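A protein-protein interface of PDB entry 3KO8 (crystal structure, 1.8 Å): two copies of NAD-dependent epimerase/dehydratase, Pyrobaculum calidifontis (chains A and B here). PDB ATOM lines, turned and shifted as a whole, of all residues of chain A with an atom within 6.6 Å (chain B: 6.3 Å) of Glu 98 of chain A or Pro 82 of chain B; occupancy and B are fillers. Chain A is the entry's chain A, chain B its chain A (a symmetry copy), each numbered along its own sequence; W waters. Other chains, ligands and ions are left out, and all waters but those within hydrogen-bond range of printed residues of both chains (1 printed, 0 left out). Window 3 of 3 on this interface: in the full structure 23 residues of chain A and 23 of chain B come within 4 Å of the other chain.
Hydrophobic or aromatic side chains of chain B within 4 Å of the printed part of chain A: Pro 82, Ile 83, Phe 86 and Val 136. Printed residues of chain A that touch a printed residue of chain B: Phe 94, Glu 98, Tyr 151 and Phe 155. Hydrophobic or aromatic side chains of chain A within 4 Å of the printed part of chain B: Phe 94, Tyr 151 and Phe 155. Among the printed residues, 6 pairs touch across the chains.
Of the printed residues of chain B, Phe 94 of chain A touches Pro 82 (3.6 Å), Ile 83 (3.3 Å) and Phe 86 (3.6 Å). Glu 98 of chain A touches just one residue of chain B: Pro 82 (3.5 Å). Of the printed residues of chain B, Phe 155 of chain A touches Val 136. Of the printed residues of chain A, Pro 82 of chain B touches Phe 94, Glu 98 and Tyr 151. The nearest printed residue of chain B that does not touch Glu 98 of chain A is Ile 83 of chain B (4.9 Å). The nearest printed residue of chain A that does not touch Pro 82 of chain B is Arg 101 of chain A (4.01 Å).
Among the printed residues, merely in contact across the chains: Phe 94 of chain A with Ile 83 of chain B, Tyr 151 of chain A with Pro 82 of chain B, Glu 98 of chain A with Pro 82 of chain B, Phe 94 of chain A with Pro 82 of chain B, Phe 94 of chain A with Phe 86 of chain B and Phe 155 of chain A with Val 136 of chain B.
No position is printed for both chains. Of the 6 pairs that touch across the chains among the printed residues, none has its exchanged pair printed and touching as well.
The side-chain hydroxyl (OH) of Tyr 55 of chain A lies within hydrogen-bond range of the side-chain carboxylate (OE2) of Glu 98 of chain A, 3.1 Å away. The guanidinium group of Arg 101 of chain A lies within salt-bridge range of the side-chain carboxylate of Glu 98 of chain A (2.8 Å). OE2 of Glu 98 of chain A is in hydrogen-bond range of NE2 of Gln 102 of chain A (3.0 Å). OE1 of Glu 98 of chain A is in hydrogen-bond range of OH of Tyr 151 of chain A (2.7 Å).
Water W1 lies within hydrogen-bond range of the side-chain carboxylate of Glu 98 of chain A, the backbone NH of Ile 83 of chain B and the side-chain hydroxyl of Tyr 55 of chain A.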
ATOM      1  N   TYR A  55     -14.205 -20.905 -11.620  1.00  0.00           N
ATOM      2  CA  TYR A  55     -14.858 -19.828 -12.346  1.00  0.00           C
ATOM      3  C   TYR A  55     -14.218 -18.475 -12.000  1.00  0.00           C
ATOM      4  O   TYR A  55     -14.078 -17.595 -12.856  1.00  0.00           O
ATOM      5  CB  TYR A  55     -16.347 -19.833 -11.977  1.00  0.00           C
ATOM      6  CG  TYR A  55     -17.187 -18.825 -12.725  1.00  0.00           C
ATOM      7  CD1 TYR A  55     -17.638 -19.078 -14.028  1.00  0.00           C
ATOM      8  CD2 TYR A  55     -17.562 -17.624 -12.115  1.00  0.00           C
ATOM      9  CE1 TYR A  55     -18.454 -18.158 -14.704  1.00  0.00           C
ATOM     10  CE2 TYR A  55     -18.370 -16.701 -12.785  1.00  0.00           C
ATOM     11  CZ  TYR A  55     -18.812 -16.980 -14.074  1.00  0.00           C
ATOM     12  OH  TYR A  55     -19.620 -16.072 -14.720  1.00  0.00           O
ATOM     13  N   TRP A  57     -11.085 -17.833 -11.303  1.00  0.00           N
ATOM     14  CA  TRP A  57      -9.642 -17.833 -11.539  1.00  0.00           C
ATOM     15  C   TRP A  57      -9.040 -16.478 -11.895  1.00  0.00           C
ATOM     16  O   TRP A  57      -7.890 -16.211 -11.553  1.00  0.00           O
ATOM     17  CB  TRP A  57      -9.282 -18.822 -12.682  1.00  0.00           C
ATOM     18  CG  TRP A  57      -9.681 -18.297 -14.048  1.00  0.00           C
ATOM     19  CD1 TRP A  57     -10.899 -18.442 -14.674  1.00  0.00           C
ATOM     20  CD2 TRP A  57      -8.906 -17.427 -14.877  1.00  0.00           C
ATOM     21  NE1 TRP A  57     -10.927 -17.704 -15.849  1.00  0.00           N
ATOM     22  CE2 TRP A  57      -9.717 -17.067 -15.993  1.00  0.00           C
ATOM     23  CE3 TRP A  57      -7.606 -16.902 -14.780  1.00  0.00           C
ATOM     24  CZ2 TRP A  57      -9.268 -16.204 -17.002  1.00  0.00           C
ATOM     25  CZ3 TRP A  57      -7.147 -16.041 -15.788  1.00  0.00           C
ATOM     26  CH2 TRP A  57      -7.985 -15.698 -16.890  1.00  0.00           C
ATOM     27  N   THR A  93     -11.757 -23.429 -20.577  1.00  0.00           N
ATOM     28  CA  THR A  93     -11.928 -22.483 -21.673  1.00  0.00           C
ATOM     29  C   THR A  93     -13.176 -21.645 -21.505  1.00  0.00           C
ATOM     30  O   THR A  93     -13.163 -20.432 -21.771  1.00  0.00           O
ATOM     31  CB  THR A  93     -11.959 -23.228 -23.019  1.00  0.00           C
ATOM     32  OG1 THR A  93     -10.671 -23.835 -23.222  1.00  0.00           O
ATOM     33  CG2 THR A  93     -12.235 -22.234 -24.182  1.00  0.00           C
ATOM     34  N   PHE A  94     -14.256 -22.265 -21.026  1.00  0.00           N
ATOM     35  CA  PHE A  94     -15.494 -21.503 -20.802  1.00  0.00           C
ATOM     36  C   PHE A  94     -15.241 -20.446 -19.723  1.00  0.00           C
ATOM     37  O   PHE A  94     -15.666 -19.269 -19.841  1.00  0.00           O
ATOM     38  CB  PHE A  94     -16.614 -22.415 -20.314  1.00  0.00           C
ATOM     39  CG  PHE A  94     -17.845 -21.653 -19.932  1.00  0.00           C
ATOM     40  CD1 PHE A  94     -18.677 -21.141 -20.923  1.00  0.00           C
ATOM     41  CD2 PHE A  94     -18.133 -21.389 -18.602  1.00  0.00           C
ATOM     42  CE1 PHE A  94     -19.789 -20.365 -20.587  1.00  0.00           C
ATOM     43  CE2 PHE A  94     -19.262 -20.599 -18.266  1.00  0.00           C
ATOM     44  CZ  PHE A  94     -20.064 -20.103 -19.269  1.00  0.00           C
ATOM     45  N   ASN A  95     -14.557 -20.863 -18.661  1.00  0.00           N
ATOM     46  CA  ASN A  95     -14.235 -19.911 -17.590  1.00  0.00           C
ATOM     47  C   ASN A  95     -13.351 -18.767 -18.099  1.00  0.00           C
ATOM     48  O   ASN A  95     -13.457 -17.639 -17.577  1.00  0.00           O
ATOM     49  CB  ASN A  95     -13.524 -20.617 -16.408  1.00  0.00           C
ATOM     50  CG  ASN A  95     -14.461 -21.548 -15.634  1.00  0.00           C
ATOM     51  OD1 ASN A  95     -15.687 -21.444 -15.731  1.00  0.00           O
ATOM     52  ND2 ASN A  95     -13.887 -22.440 -14.853  1.00  0.00           N
ATOM     53  N   VAL A  96     -12.463 -19.048 -19.055  1.00  0.00           N
ATOM     54  CA  VAL A  96     -11.617 -17.986 -19.607  1.00  0.00           C
ATOM     55  C   VAL A  96     -12.518 -17.056 -20.407  1.00  0.00           C
ATOM     56  O   VAL A  96     -12.406 -15.837 -20.315  1.00  0.00           O
ATOM     57  CB  VAL A  96     -10.500 -18.531 -20.549  1.00  0.00           C
ATOM     58  CG1 VAL A  96      -9.870 -17.392 -21.340  1.00  0.00           C
ATOM     59  CG2 VAL A  96      -9.452 -19.259 -19.720  1.00  0.00           C
ATOM     60  N   LEU A  97     -13.443 -17.608 -21.196  1.00  0.00           N
ATOM     61  CA  LEU A  97     -14.315 -16.740 -22.002  1.00  0.00           C
ATOM     62  C   LEU A  97     -15.229 -15.848 -21.134  1.00  0.00           C
ATOM     63  O   LEU A  97     -15.466 -14.669 -21.461  1.00  0.00           O
ATOM     64  CB  LEU A  97     -15.164 -17.604 -22.973  1.00  0.00           C
ATOM     65  CG  LEU A  97     -14.356 -18.343 -24.049  1.00  0.00           C
ATOM     66  CD1 LEU A  97     -15.257 -19.383 -24.788  1.00  0.00           C
ATOM     67  CD2 LEU A  97     -13.806 -17.322 -25.061  1.00  0.00           C
ATOM     68  N   GLU A  98     -15.767 -16.390 -20.044  1.00  0.00           N
ATOM     69  CA  GLU A  98     -16.599 -15.587 -19.149  1.00  0.00           C
ATOM     70  C   GLU A  98     -15.776 -14.448 -18.516  1.00  0.00           C
ATOM     71  O   GLU A  98     -16.246 -13.325 -18.370  1.00  0.00           O
ATOM     72  CB  GLU A  98     -17.181 -16.450 -18.035  1.00  0.00           C
ATOM     73  CG  GLU A  98     -18.549 -17.025 -18.410  1.00  0.00           C
ATOM     74  CD  GLU A  98     -19.566 -15.921 -18.660  1.00  0.00           C
ATOM     75  OE1 GLU A  98     -19.799 -15.573 -19.840  1.00  0.00           O
ATOM     76  OE2 GLU A  98     -20.113 -15.389 -17.660  1.00  0.00           O
ATOM     77  N   TRP A  99     -14.553 -14.750 -18.110  1.00  0.00           N
ATOM     78  CA  TRP A  99     -13.698 -13.706 -17.542  1.00  0.00           C
ATOM     79  C   TRP A  99     -13.402 -12.665 -18.625  1.00  0.00           C
ATOM     80  O   TRP A  99     -13.390 -11.449 -18.345  1.00  0.00           O
ATOM     81  CB  TRP A  99     -12.384 -14.326 -17.034  1.00  0.00           C
ATOM     82  CG  TRP A  99     -11.240 -13.341 -16.832  1.00  0.00           C
ATOM     83  CD1 TRP A  99     -10.968 -12.588 -15.711  1.00  0.00           C
ATOM     84  CD2 TRP A  99     -10.204 -13.039 -17.781  1.00  0.00           C
ATOM     85  NE1 TRP A  99      -9.815 -11.833 -15.915  1.00  0.00           N
ATOM     86  CE2 TRP A  99      -9.328 -12.096 -17.172  1.00  0.00           C
ATOM     87  CE3 TRP A  99      -9.934 -13.470 -19.078  1.00  0.00           C
ATOM     88  CZ2 TRP A  99      -8.205 -11.593 -17.820  1.00  0.00           C
ATOM     89  CZ3 TRP A  99      -8.811 -12.964 -19.736  1.00  0.00           C
ATOM     90  CH2 TRP A  99      -7.955 -12.031 -19.095  1.00  0.00           C
ATOM     91  N   ALA A 100     -13.168 -13.115 -19.858  1.00  0.00           N
ATOM     92  CA  ALA A 100     -12.867 -12.196 -20.942  1.00  0.00           C
ATOM     93  C   ALA A 100     -14.062 -11.288 -21.193  1.00  0.00           C
ATOM     94  O   ALA A 100     -13.931 -10.061 -21.358  1.00  0.00           O
ATOM     95  CB  ALA A 100     -12.520 -12.960 -22.203  1.00  0.00           C
ATOM     96  N   ARG A 101     -15.243 -11.888 -21.252  1.00  0.00           N
ATOM     97  CA  ARG A 101     -16.444 -11.088 -21.454  1.00  0.00           C
ATOM     98  C   ARG A 101     -16.673 -10.092 -20.315  1.00  0.00           C
ATOM     99  O   ARG A 101     -16.955  -8.904 -20.557  1.00  0.00           O
ATOM    100  CB  ARG A 101     -17.679 -11.998 -21.561  1.00  0.00           C
ATOM    101  CG  ARG A 101     -19.018 -11.260 -21.643  1.00  0.00           C
ATOM    102  CD  ARG A 101     -20.203 -12.267 -21.657  1.00  0.00           C
ATOM    103  NE  ARG A 101     -20.481 -12.883 -20.358  1.00  0.00           N
ATOM    104  CZ  ARG A 101     -21.177 -12.315 -19.369  1.00  0.00           C
ATOM    105  NH1 ARG A 101     -21.687 -11.098 -19.512  1.00  0.00           N
ATOM    106  NH2 ARG A 101     -21.373 -12.963 -18.229  1.00  0.00           N
ATOM    107  N   GLN A 102     -16.557 -10.557 -19.081  1.00  0.00           N
ATOM    108  CA  GLN A 102     -16.863  -9.703 -17.938  1.00  0.00           C
ATOM    109  C   GLN A 102     -15.819  -8.622 -17.685  1.00  0.00           C
ATOM    110  O   GLN A 102     -16.139  -7.594 -17.084  1.00  0.00           O
ATOM    111  CB  GLN A 102     -17.076 -10.540 -16.674  1.00  0.00           C
ATOM    112  CG  GLN A 102     -18.378 -11.392 -16.731  1.00  0.00           C
ATOM    113  CD  GLN A 102     -18.592 -12.221 -15.506  1.00  0.00           C
ATOM    114  OE1 GLN A 102     -18.454 -11.727 -14.387  1.00  0.00           O
ATOM    115  NE2 GLN A 102     -18.955 -13.497 -15.693  1.00  0.00           N
ATOM    116  N   THR A 103     -14.598  -8.826 -18.154  1.00  0.00           N
ATOM    117  CA  THR A 103     -13.577  -7.808 -17.915  1.00  0.00           C
ATOM    118  C   THR A 103     -13.287  -6.970 -19.149  1.00  0.00           C
ATOM    119  O   THR A 103     -12.405  -6.097 -19.131  1.00  0.00           O
ATOM    120  CB  THR A 103     -12.271  -8.434 -17.381  1.00  0.00           C
ATOM    121  OG1 THR A 103     -11.676  -9.271 -18.373  1.00  0.00           O
ATOM    122  CG2 THR A 103     -12.552  -9.249 -16.151  1.00  0.00           C
ATOM    123  N   TYR A 151     -18.667 -16.560 -28.552  1.00  0.00           N
ATOM    124  CA  TYR A 151     -18.435 -15.352 -27.745  1.00  0.00           C
ATOM    125  C   TYR A 151     -17.974 -14.199 -28.645  1.00  0.00           C
ATOM    126  O   TYR A 151     -18.223 -13.022 -28.320  1.00  0.00           O
ATOM    127  CB  TYR A 151     -17.394 -15.617 -26.649  1.00  0.00           C
ATOM    128  CG  TYR A 151     -18.008 -16.118 -25.358  1.00  0.00           C
ATOM    129  CD1 TYR A 151     -18.798 -17.285 -25.334  1.00  0.00           C
ATOM    130  CD2 TYR A 151     -17.862 -15.391 -24.167  1.00  0.00           C
ATOM    131  CE1 TYR A 151     -19.440 -17.698 -24.178  1.00  0.00           C
ATOM    132  CE2 TYR A 151     -18.489 -15.796 -23.002  1.00  0.00           C
ATOM    133  CZ  TYR A 151     -19.292 -16.947 -23.006  1.00  0.00           C
ATOM    134  OH  TYR A 151     -19.999 -17.273 -21.874  1.00  0.00           O
ATOM    135  N   PHE A 155     -20.711 -11.541 -28.012  1.00  0.00           N
ATOM    136  CA  PHE A 155     -20.209 -10.538 -27.084  1.00  0.00           C
ATOM    137  C   PHE A 155     -19.080  -9.654 -27.630  1.00  0.00           C
ATOM    138  O   PHE A 155     -18.606  -8.754 -26.936  1.00  0.00           O
ATOM    139  CB  PHE A 155     -19.759 -11.228 -25.797  1.00  0.00           C
ATOM    140  CG  PHE A 155     -20.834 -12.025 -25.128  1.00  0.00           C
ATOM    141  CD1 PHE A 155     -21.968 -11.397 -24.620  1.00  0.00           C
ATOM    142  CD2 PHE A 155     -20.707 -13.403 -24.967  1.00  0.00           C
ATOM    143  CE1 PHE A 155     -22.959 -12.124 -23.952  1.00  0.00           C
ATOM    144  CE2 PHE A 155     -21.682 -14.130 -24.302  1.00  0.00           C
ATOM    145  CZ  PHE A 155     -22.812 -13.499 -23.792  1.00  0.00           C
ATOM    146  N   THR B  80     -30.609 -15.602 -18.998  1.00  0.00           N
ATOM    147  CA  THR B  80     -30.064 -16.601 -18.094  1.00  0.00           C
ATOM    148  C   THR B  80     -28.539 -16.424 -18.161  1.00  0.00           C
ATOM    149  O   THR B  80     -28.018 -16.147 -19.223  1.00  0.00           O
ATOM    150  CB  THR B  80     -30.509 -18.007 -18.572  1.00  0.00           C
ATOM    151  OG1 THR B  80     -31.891 -18.177 -18.226  1.00  0.00           O
ATOM    152  CG2 THR B  80     -29.669 -19.122 -17.926  1.00  0.00           C
ATOM    153  N   GLU B  81     -27.835 -16.591 -17.042  1.00  0.00           N
ATOM    154  CA  GLU B  81     -26.368 -16.430 -17.050  1.00  0.00           C
ATOM    155  C   GLU B  81     -25.717 -17.515 -17.906  1.00  0.00           C
ATOM    156  O   GLU B  81     -26.151 -18.662 -17.887  1.00  0.00           O
ATOM    157  CB  GLU B  81     -25.813 -16.537 -15.635  1.00  0.00           C
ATOM    158  CG  GLU B  81     -26.243 -15.414 -14.707  1.00  0.00           C
ATOM    159  CD  GLU B  81     -25.531 -14.125 -15.037  1.00  0.00           C
ATOM    160  OE1 GLU B  81     -24.368 -14.191 -15.491  1.00  0.00           O
ATOM    161  OE2 GLU B  81     -26.128 -13.047 -14.839  1.00  0.00           O
ATOM    162  N   PRO B  82     -24.658 -17.163 -18.642  1.00  0.00           N
ATOM    163  CA  PRO B  82     -23.974 -18.138 -19.494  1.00  0.00           C
ATOM    164  C   PRO B  82     -23.581 -19.415 -18.746  1.00  0.00           C
ATOM    165  O   PRO B  82     -23.701 -20.510 -19.293  1.00  0.00           O
ATOM    166  CB  PRO B  82     -22.758 -17.368 -19.984  1.00  0.00           C
ATOM    167  CG  PRO B  82     -23.333 -15.945 -20.151  1.00  0.00           C
ATOM    168  CD  PRO B  82     -24.144 -15.796 -18.872  1.00  0.00           C
ATOM    169  N   ILE B  83     -23.116 -19.284 -17.503  1.00  0.00           N
ATOM    170  CA  ILE B  83     -22.678 -20.463 -16.757  1.00  0.00           C
ATOM    171  C   ILE B  83     -23.833 -21.450 -16.524  1.00  0.00           C
ATOM    172  O   ILE B  83     -23.624 -22.682 -16.429  1.00  0.00           O
ATOM    173  CB  ILE B  83     -21.986 -20.048 -15.423  1.00  0.00           C
ATOM    174  CG1 ILE B  83     -21.378 -21.284 -14.720  1.00  0.00           C
ATOM    175  CG2 ILE B  83     -22.992 -19.382 -14.531  1.00  0.00           C
ATOM    176  CD1 ILE B  83     -20.334 -21.989 -15.527  1.00  0.00           C
ATOM    177  N   VAL B  84     -25.055 -20.930 -16.454  1.00  0.00           N
ATOM    178  CA  VAL B  84     -26.211 -21.812 -16.298  1.00  0.00           C
ATOM    179  C   VAL B  84     -26.411 -22.584 -17.607  1.00  0.00           C
ATOM    180  O   VAL B  84     -26.612 -23.795 -17.576  1.00  0.00           O
ATOM    181  CB  VAL B  84     -27.488 -21.029 -15.948  1.00  0.00           C
ATOM    182  CG1 VAL B  84     -28.715 -21.971 -16.019  1.00  0.00           C
ATOM    183  CG2 VAL B  84     -27.345 -20.459 -14.531  1.00  0.00           C
ATOM    184  N   HIS B  85     -26.343 -21.898 -18.749  1.00  0.00           N
ATOM    185  CA  HIS B  85     -26.487 -22.573 -20.036  1.00  0.00           C
ATOM    186  C   HIS B  85     -25.382 -23.602 -20.170  1.00  0.00           C
ATOM    187  O   HIS B  85     -25.619 -24.718 -20.604  1.00  0.00           O
ATOM    188  CB  HIS B  85     -26.373 -21.577 -21.184  1.00  0.00           C
ATOM    189  CG  HIS B  85     -27.563 -20.687 -21.291  1.00  0.00           C
ATOM    190  ND1 HIS B  85     -27.478 -19.311 -21.405  1.00  0.00           N
ATOM    191  CD2 HIS B  85     -28.882 -20.992 -21.307  1.00  0.00           C
ATOM    192  CE1 HIS B  85     -28.701 -18.806 -21.496  1.00  0.00           C
ATOM    193  NE2 HIS B  85     -29.569 -19.806 -21.442  1.00  0.00           N
ATOM    194  N   PHE B  86     -24.170 -23.199 -19.807  1.00  0.00           N
ATOM    195  CA  PHE B  86     -23.026 -24.111 -19.900  1.00  0.00           C
ATOM    196  C   PHE B  86     -23.182 -25.356 -19.023  1.00  0.00           C
ATOM    197  O   PHE B  86     -22.973 -26.489 -19.473  1.00  0.00           O
ATOM    198  CB  PHE B  86     -21.737 -23.374 -19.489  1.00  0.00           C
ATOM    199  CG  PHE B  86     -20.506 -24.239 -19.568  1.00  0.00           C
ATOM    200  CD1 PHE B  86     -19.926 -24.539 -20.803  1.00  0.00           C
ATOM    201  CD2 PHE B  86     -19.956 -24.775 -18.413  1.00  0.00           C
ATOM    202  CE1 PHE B  86     -18.791 -25.387 -20.877  1.00  0.00           C
ATOM    203  CE2 PHE B  86     -18.834 -25.616 -18.472  1.00  0.00           C
ATOM    204  CZ  PHE B  86     -18.259 -25.918 -19.701  1.00  0.00           C
ATOM    205  N   ASN B  87     -23.529 -25.161 -17.761  1.00  0.00           N
ATOM    206  CA  ASN B  87     -23.638 -26.279 -16.854  1.00  0.00           C
ATOM    207  C   ASN B  87     -24.792 -27.205 -17.175  1.00  0.00           C
ATOM    208  O   ASN B  87     -24.623 -28.431 -17.113  1.00  0.00           O
ATOM    209  CB  ASN B  87     -23.798 -25.783 -15.417  1.00  0.00           C
ATOM    210  CG  ASN B  87     -22.488 -25.288 -14.822  1.00  0.00           C
ATOM    211  OD1 ASN B  87     -21.415 -25.508 -15.373  1.00  0.00           O
ATOM    212  ND2 ASN B  87     -22.583 -24.627 -13.668  1.00  0.00           N
ATOM    213  N   VAL B 136     -25.257 -18.607 -26.183  1.00  0.00           N
ATOM    214  CA  VAL B 136     -24.432 -19.538 -25.433  1.00  0.00           C
ATOM    215  C   VAL B 136     -25.146 -20.911 -25.454  1.00  0.00           C
ATOM    216  O   VAL B 136     -24.490 -21.975 -25.499  1.00  0.00           O
ATOM    217  CB  VAL B 136     -24.256 -19.060 -23.990  1.00  0.00           C
ATOM    218  CG1 VAL B 136     -23.489 -20.123 -23.167  1.00  0.00           C
ATOM    219  CG2 VAL B 136     -23.461 -17.700 -24.007  1.00  0.00           C
HETATM  220  O   HOH W   1     -22.005 -16.737 -16.399  1.00  0.00           O
